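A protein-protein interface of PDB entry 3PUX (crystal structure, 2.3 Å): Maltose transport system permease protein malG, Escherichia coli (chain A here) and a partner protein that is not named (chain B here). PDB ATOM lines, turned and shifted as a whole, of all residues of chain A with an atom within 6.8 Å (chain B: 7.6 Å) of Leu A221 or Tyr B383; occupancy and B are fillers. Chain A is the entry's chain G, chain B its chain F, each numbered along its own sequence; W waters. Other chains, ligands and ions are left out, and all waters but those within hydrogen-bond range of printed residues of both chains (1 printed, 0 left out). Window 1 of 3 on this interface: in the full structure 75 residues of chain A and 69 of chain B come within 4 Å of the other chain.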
ATOM      1  N   LEU A 172     -40.398 -12.670 -23.003  1.00  0.00           N
ATOM      2  CA  LEU A 172     -39.815 -12.987 -24.278  1.00  0.00           C
ATOM      3  C   LEU A 172     -39.187 -14.368 -24.252  1.00  0.00           C
ATOM      4  O   LEU A 172     -39.267 -15.129 -25.246  1.00  0.00           O
ATOM      5  CB  LEU A 172     -38.794 -11.908 -24.680  1.00  0.00           C
ATOM      6  CG  LEU A 172     -39.418 -10.688 -25.387  1.00  0.00           C
ATOM      7  CD1 LEU A 172     -38.420  -9.580 -25.609  1.00  0.00           C
ATOM      8  CD2 LEU A 172     -40.021 -11.135 -26.704  1.00  0.00           C
ATOM      9  N   HIS A 173     -38.573 -14.689 -23.111  1.00  0.00           N
ATOM     10  CA  HIS A 173     -37.941 -15.975 -22.891  1.00  0.00           C
ATOM     11  C   HIS A 173     -39.033 -17.058 -22.910  1.00  0.00           C
ATOM     12  O   HIS A 173     -38.847 -18.155 -23.496  1.00  0.00           O
ATOM     13  CB  HIS A 173     -37.193 -15.957 -21.566  1.00  0.00           C
ATOM     14  CG  HIS A 173     -36.060 -14.976 -21.506  1.00  0.00           C
ATOM     15  ND1 HIS A 173     -35.026 -14.966 -22.423  1.00  0.00           N
ATOM     16  CD2 HIS A 173     -35.743 -14.034 -20.580  1.00  0.00           C
ATOM     17  CE1 HIS A 173     -34.146 -14.030 -22.092  1.00  0.00           C
ATOM     18  NE2 HIS A 173     -34.553 -13.452 -20.974  1.00  0.00           N
ATOM     19  N   THR A 176     -39.801 -17.680 -26.479  1.00  0.00           N
ATOM     20  CA  THR A 176     -38.648 -18.382 -27.055  1.00  0.00           C
ATOM     21  C   THR A 176     -38.645 -19.869 -26.711  1.00  0.00           C
ATOM     22  O   THR A 176     -38.394 -20.703 -27.563  1.00  0.00           O
ATOM     23  CB  THR A 176     -37.314 -17.787 -26.564  1.00  0.00           C
ATOM     24  OG1 THR A 176     -37.281 -16.382 -26.842  1.00  0.00           O
ATOM     25  CG2 THR A 176     -36.104 -18.501 -27.214  1.00  0.00           C
ATOM     26  N   ALA A 216     -29.950 -23.100 -22.905  1.00  0.00           N
ATOM     27  CA  ALA A 216     -28.656 -22.439 -22.817  1.00  0.00           C
ATOM     28  C   ALA A 216     -28.827 -21.018 -23.331  1.00  0.00           C
ATOM     29  O   ALA A 216     -28.297 -20.087 -22.746  1.00  0.00           O
ATOM     30  CB  ALA A 216     -27.554 -23.210 -23.604  1.00  0.00           C
ATOM     31  N   VAL A 217     -29.606 -20.862 -24.399  1.00  0.00           N
ATOM     32  CA  VAL A 217     -29.839 -19.551 -24.979  1.00  0.00           C
ATOM     33  C   VAL A 217     -30.428 -18.593 -23.945  1.00  0.00           C
ATOM     34  O   VAL A 217     -29.860 -17.530 -23.710  1.00  0.00           O
ATOM     35  CB  VAL A 217     -30.762 -19.609 -26.219  1.00  0.00           C
ATOM     36  CG1 VAL A 217     -31.401 -18.205 -26.540  1.00  0.00           C
ATOM     37  CG2 VAL A 217     -30.028 -20.187 -27.401  1.00  0.00           C
ATOM     38  N   VAL A 218     -31.548 -18.960 -23.331  1.00  0.00           N
ATOM     39  CA  VAL A 218     -32.165 -18.097 -22.323  1.00  0.00           C
ATOM     40  C   VAL A 218     -31.260 -17.850 -21.105  1.00  0.00           C
ATOM     41  O   VAL A 218     -31.232 -16.738 -20.564  1.00  0.00           O
ATOM     42  CB  VAL A 218     -33.608 -18.607 -21.876  1.00  0.00           C
ATOM     43  CG1 VAL A 218     -34.153 -17.752 -20.772  1.00  0.00           C
ATOM     44  CG2 VAL A 218     -34.579 -18.572 -23.032  1.00  0.00           C
ATOM     45  N   PHE A 219     -30.508 -18.864 -20.685  1.00  0.00           N
ATOM     46  CA  PHE A 219     -29.490 -18.655 -19.630  1.00  0.00           C
ATOM     47  C   PHE A 219     -28.434 -17.624 -20.008  1.00  0.00           C
ATOM     48  O   PHE A 219     -27.983 -16.812 -19.171  1.00  0.00           O
ATOM     49  CB  PHE A 219     -28.777 -19.941 -19.214  1.00  0.00           C
ATOM     50  CG  PHE A 219     -27.882 -19.758 -18.011  1.00  0.00           C
ATOM     51  CD1 PHE A 219     -28.367 -19.972 -16.725  1.00  0.00           C
ATOM     52  CD2 PHE A 219     -26.553 -19.362 -18.160  1.00  0.00           C
ATOM     53  CE1 PHE A 219     -27.567 -19.801 -15.616  1.00  0.00           C
ATOM     54  CE2 PHE A 219     -25.737 -19.172 -17.035  1.00  0.00           C
ATOM     55  CZ  PHE A 219     -26.250 -19.389 -15.764  1.00  0.00           C
ATOM     56  N   ILE A 220     -28.027 -17.665 -21.265  1.00  0.00           N
ATOM     57  CA  ILE A 220     -26.999 -16.752 -21.729  1.00  0.00           C
ATOM     58  C   ILE A 220     -27.576 -15.365 -21.863  1.00  0.00           C
ATOM     59  O   ILE A 220     -27.025 -14.419 -21.305  1.00  0.00           O
ATOM     60  CB  ILE A 220     -26.432 -17.196 -23.067  1.00  0.00           C
ATOM     61  CG1 ILE A 220     -25.503 -18.392 -22.862  1.00  0.00           C
ATOM     62  CG2 ILE A 220     -25.824 -16.000 -23.806  1.00  0.00           C
ATOM     63  CD1 ILE A 220     -25.425 -19.257 -24.103  1.00  0.00           C
ATOM     64  N   LEU A 221     -28.680 -15.234 -22.598  1.00  0.00           N
ATOM     65  CA  LEU A 221     -29.294 -13.936 -22.806  1.00  0.00           C
ATOM     66  C   LEU A 221     -29.651 -13.234 -21.490  1.00  0.00           C
ATOM     67  O   LEU A 221     -29.646 -12.013 -21.418  1.00  0.00           O
ATOM     68  CB  LEU A 221     -30.513 -14.049 -23.680  1.00  0.00           C
ATOM     69  CG  LEU A 221     -30.217 -14.268 -25.169  1.00  0.00           C
ATOM     70  CD1 LEU A 221     -31.525 -14.297 -25.925  1.00  0.00           C
ATOM     71  CD2 LEU A 221     -29.256 -13.206 -25.796  1.00  0.00           C
ATOM     72  N   SER A 222     -29.922 -14.020 -20.453  1.00  0.00           N
ATOM     73  CA  SER A 222     -30.230 -13.477 -19.135  1.00  0.00           C
ATOM     74  C   SER A 222     -29.037 -13.065 -18.342  1.00  0.00           C
ATOM     75  O   SER A 222     -29.074 -12.063 -17.648  1.00  0.00           O
ATOM     76  CB  SER A 222     -30.970 -14.515 -18.332  1.00  0.00           C
ATOM     77  OG  SER A 222     -32.164 -14.711 -18.993  1.00  0.00           O
ATOM     78  N   PHE A 223     -27.995 -13.878 -18.394  1.00  0.00           N
ATOM     79  CA  PHE A 223     -26.763 -13.563 -17.711  1.00  0.00           C
ATOM     80  C   PHE A 223     -26.195 -12.229 -18.248  1.00  0.00           C
ATOM     81  O   PHE A 223     -25.818 -11.380 -17.476  1.00  0.00           O
ATOM     82  CB  PHE A 223     -25.781 -14.717 -17.889  1.00  0.00           C
ATOM     83  CG  PHE A 223     -24.618 -14.658 -16.976  1.00  0.00           C
ATOM     84  CD1 PHE A 223     -24.689 -15.226 -15.721  1.00  0.00           C
ATOM     85  CD2 PHE A 223     -23.442 -14.044 -17.372  1.00  0.00           C
ATOM     86  CE1 PHE A 223     -23.595 -15.200 -14.852  1.00  0.00           C
ATOM     87  CE2 PHE A 223     -22.341 -14.007 -16.525  1.00  0.00           C
ATOM     88  CZ  PHE A 223     -22.418 -14.585 -15.255  1.00  0.00           C
ATOM     89  N   ILE A 224     -26.155 -12.060 -19.568  1.00  0.00           N
ATOM     90  CA  ILE A 224     -25.682 -10.832 -20.206  1.00  0.00           C
ATOM     91  C   ILE A 224     -26.472  -9.621 -19.745  1.00  0.00           C
ATOM     92  O   ILE A 224     -25.889  -8.633 -19.308  1.00  0.00           O
ATOM     93  CB  ILE A 224     -25.753 -10.922 -21.731  1.00  0.00           C
ATOM     94  CG1 ILE A 224     -24.742 -11.946 -22.247  1.00  0.00           C
ATOM     95  CG2 ILE A 224     -25.498  -9.565 -22.361  1.00  0.00           C
ATOM     96  CD1 ILE A 224     -24.902 -12.251 -23.717  1.00  0.00           C
ATOM     97  N   ALA A 225     -27.801  -9.716 -19.840  1.00  0.00           N
ATOM     98  CA  ALA A 225     -28.699  -8.666 -19.414  1.00  0.00           C
ATOM     99  C   ALA A 225     -28.364  -8.217 -17.992  1.00  0.00           C
ATOM    100  O   ALA A 225     -28.235  -7.015 -17.733  1.00  0.00           O
ATOM    101  CB  ALA A 225     -30.115  -9.148 -19.497  1.00  0.00           C
ATOM    102  N   ALA A 226     -28.226  -9.192 -17.090  1.00  0.00           N
ATOM    103  CA  ALA A 226     -27.945  -8.950 -15.671  1.00  0.00           C
ATOM    104  C   ALA A 226     -26.594  -8.299 -15.397  1.00  0.00           C
ATOM    105  O   ALA A 226     -26.477  -7.404 -14.523  1.00  0.00           O
ATOM    106  CB  ALA A 226     -28.078 -10.244 -14.873  1.00  0.00           C
ATOM    107  N   THR B 295     -29.901  -7.146 -38.284  1.00  0.00           N
ATOM    108  CA  THR B 295     -29.465  -7.940 -37.127  1.00  0.00           C
ATOM    109  C   THR B 295     -29.916  -9.398 -37.233  1.00  0.00           C
ATOM    110  O   THR B 295     -29.128 -10.301 -36.987  1.00  0.00           O
ATOM    111  CB  THR B 295     -29.859  -7.313 -35.771  1.00  0.00           C
ATOM    112  OG1 THR B 295     -31.275  -7.060 -35.729  1.00  0.00           O
ATOM    113  CG2 THR B 295     -29.106  -6.001 -35.574  1.00  0.00           C
ATOM    114  N   VAL B 296     -31.163  -9.631 -37.625  1.00  0.00           N
ATOM    115  CA  VAL B 296     -31.657 -11.002 -37.843  1.00  0.00           C
ATOM    116  C   VAL B 296     -30.836 -11.676 -38.938  1.00  0.00           C
ATOM    117  O   VAL B 296     -30.388 -12.807 -38.766  1.00  0.00           O
ATOM    118  CB  VAL B 296     -33.182 -11.023 -38.178  1.00  0.00           C
ATOM    119  CG1 VAL B 296     -33.664 -12.400 -38.629  1.00  0.00           C
ATOM    120  CG2 VAL B 296     -34.001 -10.573 -36.968  1.00  0.00           C
ATOM    121  N   GLY B 299     -27.005 -12.075 -37.948  1.00  0.00           N
ATOM    122  CA  GLY B 299     -26.929 -13.048 -36.866  1.00  0.00           C
ATOM    123  C   GLY B 299     -27.267 -14.465 -37.310  1.00  0.00           C
ATOM    124  O   GLY B 299     -26.589 -15.433 -36.924  1.00  0.00           O
ATOM    125  N   LEU B 321     -17.346 -13.405 -32.011  1.00  0.00           N
ATOM    126  CA  LEU B 321     -18.467 -12.754 -32.677  1.00  0.00           C
ATOM    127  C   LEU B 321     -19.526 -12.184 -31.720  1.00  0.00           C
ATOM    128  O   LEU B 321     -20.336 -11.349 -32.141  1.00  0.00           O
ATOM    129  CB  LEU B 321     -19.118 -13.690 -33.703  1.00  0.00           C
ATOM    130  CG  LEU B 321     -18.303 -13.932 -34.973  1.00  0.00           C
ATOM    131  CD1 LEU B 321     -18.767 -15.175 -35.716  1.00  0.00           C
ATOM    132  CD2 LEU B 321     -18.301 -12.687 -35.886  1.00  0.00           C
ATOM    133  N   ILE B 322     -19.529 -12.625 -30.460  1.00  0.00           N
ATOM    134  CA  ILE B 322     -20.475 -12.082 -29.476  1.00  0.00           C
ATOM    135  C   ILE B 322     -19.881 -10.994 -28.560  1.00  0.00           C
ATOM    136  O   ILE B 322     -20.598 -10.314 -27.832  1.00  0.00           O
ATOM    137  CB  ILE B 322     -21.186 -13.208 -28.650  1.00  0.00           C
ATOM    138  CG1 ILE B 322     -20.200 -14.115 -27.909  1.00  0.00           C
ATOM    139  CG2 ILE B 322     -22.058 -14.090 -29.563  1.00  0.00           C
ATOM    140  CD1 ILE B 322     -19.820 -13.630 -26.554  1.00  0.00           C
ATOM    141  N   TYR B 325     -21.327  -7.788 -27.432  1.00  0.00           N
ATOM    142  CA  TYR B 325     -22.472  -7.825 -26.533  1.00  0.00           C
ATOM    143  C   TYR B 325     -22.026  -8.112 -25.104  1.00  0.00           C
ATOM    144  O   TYR B 325     -22.785  -7.921 -24.161  1.00  0.00           O
ATOM    145  CB  TYR B 325     -23.440  -8.890 -27.025  1.00  0.00           C
ATOM    146  CG  TYR B 325     -24.855  -8.867 -26.466  1.00  0.00           C
ATOM    147  CD1 TYR B 325     -25.459  -7.680 -26.003  1.00  0.00           C
ATOM    148  CD2 TYR B 325     -25.616 -10.037 -26.461  1.00  0.00           C
ATOM    149  CE1 TYR B 325     -26.793  -7.691 -25.524  1.00  0.00           C
ATOM    150  CE2 TYR B 325     -26.924 -10.060 -25.990  1.00  0.00           C
ATOM    151  CZ  TYR B 325     -27.505  -8.900 -25.527  1.00  0.00           C
ATOM    152  OH  TYR B 325     -28.798  -8.987 -25.084  1.00  0.00           O
ATOM    153  N   THR B 377     -26.489  -2.213 -35.713  1.00  0.00           N
ATOM    154  CA  THR B 377     -26.266  -3.582 -36.190  1.00  0.00           C
ATOM    155  C   THR B 377     -25.117  -4.298 -35.439  1.00  0.00           C
ATOM    156  O   THR B 377     -25.186  -5.519 -35.198  1.00  0.00           O
ATOM    157  CB  THR B 377     -25.941  -3.590 -37.706  1.00  0.00           C
ATOM    158  OG1 THR B 377     -27.007  -2.972 -38.445  1.00  0.00           O
ATOM    159  CG2 THR B 377     -25.719  -5.013 -38.219  1.00  0.00           C
ATOM    160  N   TRP B 378     -24.065  -3.535 -35.113  1.00  0.00           N
ATOM    161  CA  TRP B 378     -22.891  -4.017 -34.388  1.00  0.00           C
ATOM    162  C   TRP B 378     -23.316  -4.374 -32.969  1.00  0.00           C
ATOM    163  O   TRP B 378     -22.933  -5.410 -32.432  1.00  0.00           O
ATOM    164  CB  TRP B 378     -21.819  -2.919 -34.355  1.00  0.00           C
ATOM    165  CG  TRP B 378     -20.509  -3.300 -33.723  1.00  0.00           C
ATOM    166  CD1 TRP B 378     -19.403  -3.812 -34.358  1.00  0.00           C
ATOM    167  CD2 TRP B 378     -20.144  -3.164 -32.342  1.00  0.00           C
ATOM    168  NE1 TRP B 378     -18.374  -3.994 -33.461  1.00  0.00           N
ATOM    169  CE2 TRP B 378     -18.800  -3.610 -32.217  1.00  0.00           C
ATOM    170  CE3 TRP B 378     -20.818  -2.696 -31.197  1.00  0.00           C
ATOM    171  CZ2 TRP B 378     -18.127  -3.624 -30.992  1.00  0.00           C
ATOM    172  CZ3 TRP B 378     -20.152  -2.699 -29.992  1.00  0.00           C
ATOM    173  CH2 TRP B 378     -18.804  -3.149 -29.900  1.00  0.00           C
ATOM    174  N   LEU B 379     -24.112  -3.505 -32.362  1.00  0.00           N
ATOM    175  CA  LEU B 379     -24.668  -3.772 -31.035  1.00  0.00           C
ATOM    176  C   LEU B 379     -25.660  -4.948 -31.028  1.00  0.00           C
ATOM    177  O   LEU B 379     -25.708  -5.712 -30.071  1.00  0.00           O
ATOM    178  CB  LEU B 379     -25.372  -2.522 -30.489  1.00  0.00           C
ATOM    179  CG  LEU B 379     -24.619  -1.215 -30.218  1.00  0.00           C
ATOM    180  CD1 LEU B 379     -25.628  -0.100 -29.911  1.00  0.00           C
ATOM    181  CD2 LEU B 379     -23.649  -1.381 -29.076  1.00  0.00           C
ATOM    182  N   GLY B 380     -26.450  -5.095 -32.088  1.00  0.00           N
ATOM    183  CA  GLY B 380     -27.623  -5.994 -32.041  1.00  0.00           C
ATOM    184  C   GLY B 380     -27.512  -7.379 -32.658  1.00  0.00           C
ATOM    185  O   GLY B 380     -28.344  -8.248 -32.381  1.00  0.00           O
ATOM    186  N   TYR B 381     -26.503  -7.592 -33.488  1.00  0.00           N
ATOM    187  CA  TYR B 381     -26.359  -8.883 -34.166  1.00  0.00           C
ATOM    188  C   TYR B 381     -26.071 -10.076 -33.222  1.00  0.00           C
ATOM    189  O   TYR B 381     -26.568 -11.170 -33.482  1.00  0.00           O
ATOM    190  CB  TYR B 381     -25.371  -8.822 -35.356  1.00  0.00           C
ATOM    191  CG  TYR B 381     -23.909  -9.039 -35.007  1.00  0.00           C
ATOM    192  CD1 TYR B 381     -23.412 -10.323 -34.742  1.00  0.00           C
ATOM    193  CD2 TYR B 381     -23.028  -7.970 -34.974  1.00  0.00           C
ATOM    194  CE1 TYR B 381     -22.070 -10.531 -34.435  1.00  0.00           C
ATOM    195  CE2 TYR B 381     -21.681  -8.148 -34.656  1.00  0.00           C
ATOM    196  CZ  TYR B 381     -21.208  -9.430 -34.389  1.00  0.00           C
ATOM    197  OH  TYR B 381     -19.887  -9.604 -34.054  1.00  0.00           O
ATOM    198  N   PRO B 382     -25.288  -9.875 -32.130  1.00  0.00           N
ATOM    199  CA  PRO B 382     -25.027 -11.015 -31.240  1.00  0.00           C
ATOM    200  C   PRO B 382     -26.274 -11.613 -30.612  1.00  0.00           C
ATOM    201  O   PRO B 382     -26.376 -12.836 -30.473  1.00  0.00           O
ATOM    202  CB  PRO B 382     -24.107 -10.415 -30.179  1.00  0.00           C
ATOM    203  CG  PRO B 382     -23.340  -9.363 -30.946  1.00  0.00           C
ATOM    204  CD  PRO B 382     -24.435  -8.721 -31.762  1.00  0.00           C
ATOM    205  N   TYR B 383     -27.213 -10.745 -30.252  1.00  0.00           N
ATOM    206  CA  TYR B 383     -28.489 -11.133 -29.690  1.00  0.00           C
ATOM    207  C   TYR B 383     -29.232 -12.045 -30.660  1.00  0.00           C
ATOM    208  O   TYR B 383     -29.683 -13.121 -30.279  1.00  0.00           O
ATOM    209  CB  TYR B 383     -29.314  -9.875 -29.408  1.00  0.00           C
ATOM    210  CG  TYR B 383     -30.723 -10.131 -28.936  1.00  0.00           C
ATOM    211  CD1 TYR B 383     -30.971 -10.670 -27.673  1.00  0.00           C
ATOM    212  CD2 TYR B 383     -31.816  -9.826 -29.749  1.00  0.00           C
ATOM    213  CE1 TYR B 383     -32.274 -10.915 -27.234  1.00  0.00           C
ATOM    214  CE2 TYR B 383     -33.144 -10.047 -29.307  1.00  0.00           C
ATOM    215  CZ  TYR B 383     -33.361 -10.583 -28.049  1.00  0.00           C
ATOM    216  OH  TYR B 383     -34.651 -10.819 -27.615  1.00  0.00           O
ATOM    217  N   MET B 384     -29.349 -11.621 -31.917  1.00  0.00           N
ATOM    218  CA  MET B 384     -30.023 -12.430 -32.922  1.00  0.00           C
ATOM    219  C   MET B 384     -29.251 -13.670 -33.248  1.00  0.00           C
ATOM    220  O   MET B 384     -29.858 -14.723 -33.456  1.00  0.00           O
ATOM    221  CB  MET B 384     -30.285 -11.638 -34.180  1.00  0.00           C
ATOM    222  CG  MET B 384     -31.366 -10.609 -34.017  1.00  0.00           C
ATOM    223  SD  MET B 384     -32.930 -11.364 -33.528  1.00  0.00           S
ATOM    224  CE  MET B 384     -33.877  -9.858 -33.243  1.00  0.00           C
ATOM    225  N   MET B 385     -27.920 -13.557 -33.298  1.00  0.00           N
ATOM    226  CA  MET B 385     -27.038 -14.728 -33.408  1.00  0.00           C
ATOM    227  C   MET B 385     -27.258 -15.804 -32.336  1.00  0.00           C
ATOM    228  O   MET B 385     -27.439 -16.974 -32.647  1.00  0.00           O
ATOM    229  CB  MET B 385     -25.574 -14.311 -33.370  1.00  0.00           C
ATOM    230  CG  MET B 385     -24.634 -15.471 -33.712  1.00  0.00           C
ATOM    231  SD  MET B 385     -22.937 -14.947 -33.583  1.00  0.00           S
ATOM    232  CE  MET B 385     -22.095 -16.464 -34.056  1.00  0.00           C
ATOM    233  N   ILE B 386     -27.234 -15.394 -31.074  1.00  0.00           N
ATOM    234  CA  ILE B 386     -27.363 -16.344 -29.975  1.00  0.00           C
ATOM    235  C   ILE B 386     -28.709 -17.093 -30.010  1.00  0.00           C
ATOM    236  O   ILE B 386     -28.758 -18.301 -29.786  1.00  0.00           O
ATOM    237  CB  ILE B 386     -27.147 -15.663 -28.601  1.00  0.00           C
ATOM    238  CG1 ILE B 386     -25.713 -15.138 -28.483  1.00  0.00           C
ATOM    239  CG2 ILE B 386     -27.392 -16.669 -27.488  1.00  0.00           C
ATOM    240  CD1 ILE B 386     -25.528 -14.051 -27.394  1.00  0.00           C
ATOM    241  N   LEU B 387     -29.782 -16.355 -30.288  1.00  0.00           N
ATOM    242  CA  LEU B 387     -31.089 -16.943 -30.521  1.00  0.00           C
ATOM    243  C   LEU B 387     -31.012 -17.992 -31.628  1.00  0.00           C
ATOM    244  O   LEU B 387     -31.392 -19.134 -31.432  1.00  0.00           O
ATOM    245  CB  LEU B 387     -32.083 -15.852 -30.899  1.00  0.00           C
ATOM    246  CG  LEU B 387     -32.580 -14.996 -29.742  1.00  0.00           C
ATOM    247  CD1 LEU B 387     -33.378 -13.871 -30.322  1.00  0.00           C
ATOM    248  CD2 LEU B 387     -33.440 -15.837 -28.797  1.00  0.00           C
ATOM    249  N   CYS B 388     -30.490 -17.612 -32.779  1.00  0.00           N
ATOM    250  CA  CYS B 388     -30.369 -18.550 -33.869  1.00  0.00           C
ATOM    251  C   CYS B 388     -29.510 -19.760 -33.551  1.00  0.00           C
ATOM    252  O   CYS B 388     -29.861 -20.876 -33.952  1.00  0.00           O
ATOM    253  CB  CYS B 388     -29.932 -17.856 -35.143  1.00  0.00           C
ATOM    254  SG  CYS B 388     -31.237 -16.734 -35.698  1.00  0.00           S
ATOM    255  N   MET B 389     -28.442 -19.562 -32.779  1.00  0.00           N
ATOM    256  CA  MET B 389     -27.555 -20.670 -32.398  1.00  0.00           C
ATOM    257  C   MET B 389     -28.355 -21.759 -31.706  1.00  0.00           C
ATOM    258  O   MET B 389     -28.167 -22.944 -31.952  1.00  0.00           O
ATOM    259  CB  MET B 389     -26.402 -20.189 -31.521  1.00  0.00           C
ATOM    260  CG  MET B 389     -25.312 -19.431 -32.281  1.00  0.00           C
ATOM    261  SD  MET B 389     -24.020 -18.785 -31.198  1.00  0.00           S
ATOM    262  CE  MET B 389     -23.749 -20.241 -30.159  1.00  0.00           C
ATOM    263  N   PRO B 428     -42.052 -13.604 -32.997  1.00  0.00           N
ATOM    264  CA  PRO B 428     -42.257 -12.784 -31.801  1.00  0.00           C
ATOM    265  C   PRO B 428     -41.012 -11.994 -31.419  1.00  0.00           C
ATOM    266  O   PRO B 428     -41.125 -10.794 -31.172  1.00  0.00           O
ATOM    267  CB  PRO B 428     -42.621 -13.799 -30.702  1.00  0.00           C
ATOM    268  CG  PRO B 428     -42.318 -15.164 -31.290  1.00  0.00           C
ATOM    269  CD  PRO B 428     -42.444 -15.012 -32.779  1.00  0.00           C
ATOM    270  N   LEU B 429     -39.838 -12.635 -31.404  1.00  0.00           N
ATOM    271  CA  LEU B 429     -38.585 -11.924 -31.098  1.00  0.00           C
ATOM    272  C   LEU B 429     -38.305 -10.747 -32.024  1.00  0.00           C
ATOM    273  O   LEU B 429     -37.750  -9.734 -31.583  1.00  0.00           O
ATOM    274  CB  LEU B 429     -37.397 -12.872 -31.059  1.00  0.00           C
ATOM    275  CG  LEU B 429     -37.616 -13.959 -30.015  1.00  0.00           C
ATOM    276  CD1 LEU B 429     -36.767 -15.193 -30.290  1.00  0.00           C
ATOM    277  CD2 LEU B 429     -37.427 -13.421 -28.590  1.00  0.00           C
ATOM    278  N   MET B 430     -38.719 -10.861 -33.285  1.00  0.00           N
ATOM    279  CA  MET B 430     -38.530  -9.764 -34.233  1.00  0.00           C
ATOM    280  C   MET B 430     -39.504  -8.612 -33.976  1.00  0.00           C
ATOM    281  O   MET B 430     -39.105  -7.452 -34.026  1.00  0.00           O
ATOM    282  CB  MET B 430     -38.611 -10.242 -35.685  1.00  0.00           C
ATOM    283  CG  MET B 430     -37.449 -11.108 -36.129  1.00  0.00           C
ATOM    284  SD  MET B 430     -37.708 -11.872 -37.751  1.00  0.00           S
ATOM    285  CE  MET B 430     -37.509 -10.426 -38.813  1.00  0.00           C
ATOM    286  N   ALA B 432     -40.732  -7.859 -31.217  1.00  0.00           N
ATOM    287  CA  ALA B 432     -40.299  -7.238 -29.974  1.00  0.00           C
ATOM    288  C   ALA B 432     -39.073  -6.369 -30.187  1.00  0.00           C
ATOM    289  O   ALA B 432     -38.916  -5.301 -29.577  1.00  0.00           O
ATOM    290  CB  ALA B 432     -40.024  -8.289 -28.967  1.00  0.00           C
ATOM    291  N   SER B 433     -38.189  -6.826 -31.061  1.00  0.00           N
ATOM    292  CA  SER B 433     -36.976  -6.074 -31.351  1.00  0.00           C
ATOM    293  C   SER B 433     -37.325  -4.771 -32.062  1.00  0.00           C
ATOM    294  O   SER B 433     -36.629  -3.786 -31.915  1.00  0.00           O
ATOM    295  CB  SER B 433     -36.013  -6.914 -32.190  1.00  0.00           C
ATOM    296  OG  SER B 433     -34.830  -6.193 -32.481  1.00  0.00           O
HETATM  297  O   HOH W   1     -30.139  -9.882 -23.180  1.00  0.00           O
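O of Leu A172 is in hydrogen-bond range of OG1 of Thr A176 (2.8 Å).
Among the printed residues, pairs that only touch across the chains: Val A217 with Ile B386 (3.3 Å), Thr A176 with Leu B429 (3.4 Å), Leu A221 with Tyr B383 (3.6 Å), Ile A224 with Tyr B325 (3.6 Å), Leu A172 with Ala B432 (3.6 Å), Leu A221 with Leu B387 (3.8 Å), Val A217 with Leu B387 (3.9 Å), Leu A221 with Tyr B325 (3.9 Å) and Leu A172 with Leu B429 (3.9 Å).
Of the printed residues of chain B, Thr A176 touches Leu B429. Of the printed residues of chain B, Val A217 touches Ile B386 (3.3 Å) and Leu B387 (3.9 Å). Of chain B, only Tyr B325, Tyr B383 and Leu B387 come within 4 Å of Leu A221. Printed residues of chain B within 4 Å of Ile A224: Tyr B325. Of the printed residues of chain A, Tyr B325 touches Leu A221 and Ile A224. Printed residues of chain A within 4 Å of Tyr B383: Leu A221. Printed residues of chain A within 4 Å of Ile B386: Val A217 (3.3 Å). The nearest residue of chain A that does not touch Tyr B383 is Leu A172 (4.4 Å).
Of the 24 printed residues of chain B, 6 touch a printed residue of chain A. Printed residues of chain A that touch a printed residue of chain B: Leu A172, Thr A176, Val A217, Leu A221 and Ile A224. Hydrophobic or aromatic side chains of chain A within 4 Å of the printed part of chain B: Leu A172, Val A217, Leu A221 and Ile A224. Among the printed residues, no Asp or Glu carboxylate lies within 4 Å of a Lys or Arg side-chain nitrogen of the other chain.
Water W1 bridges OH of Tyr B325 (2.5 Å) and O of Leu A221 (2.8 Å).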
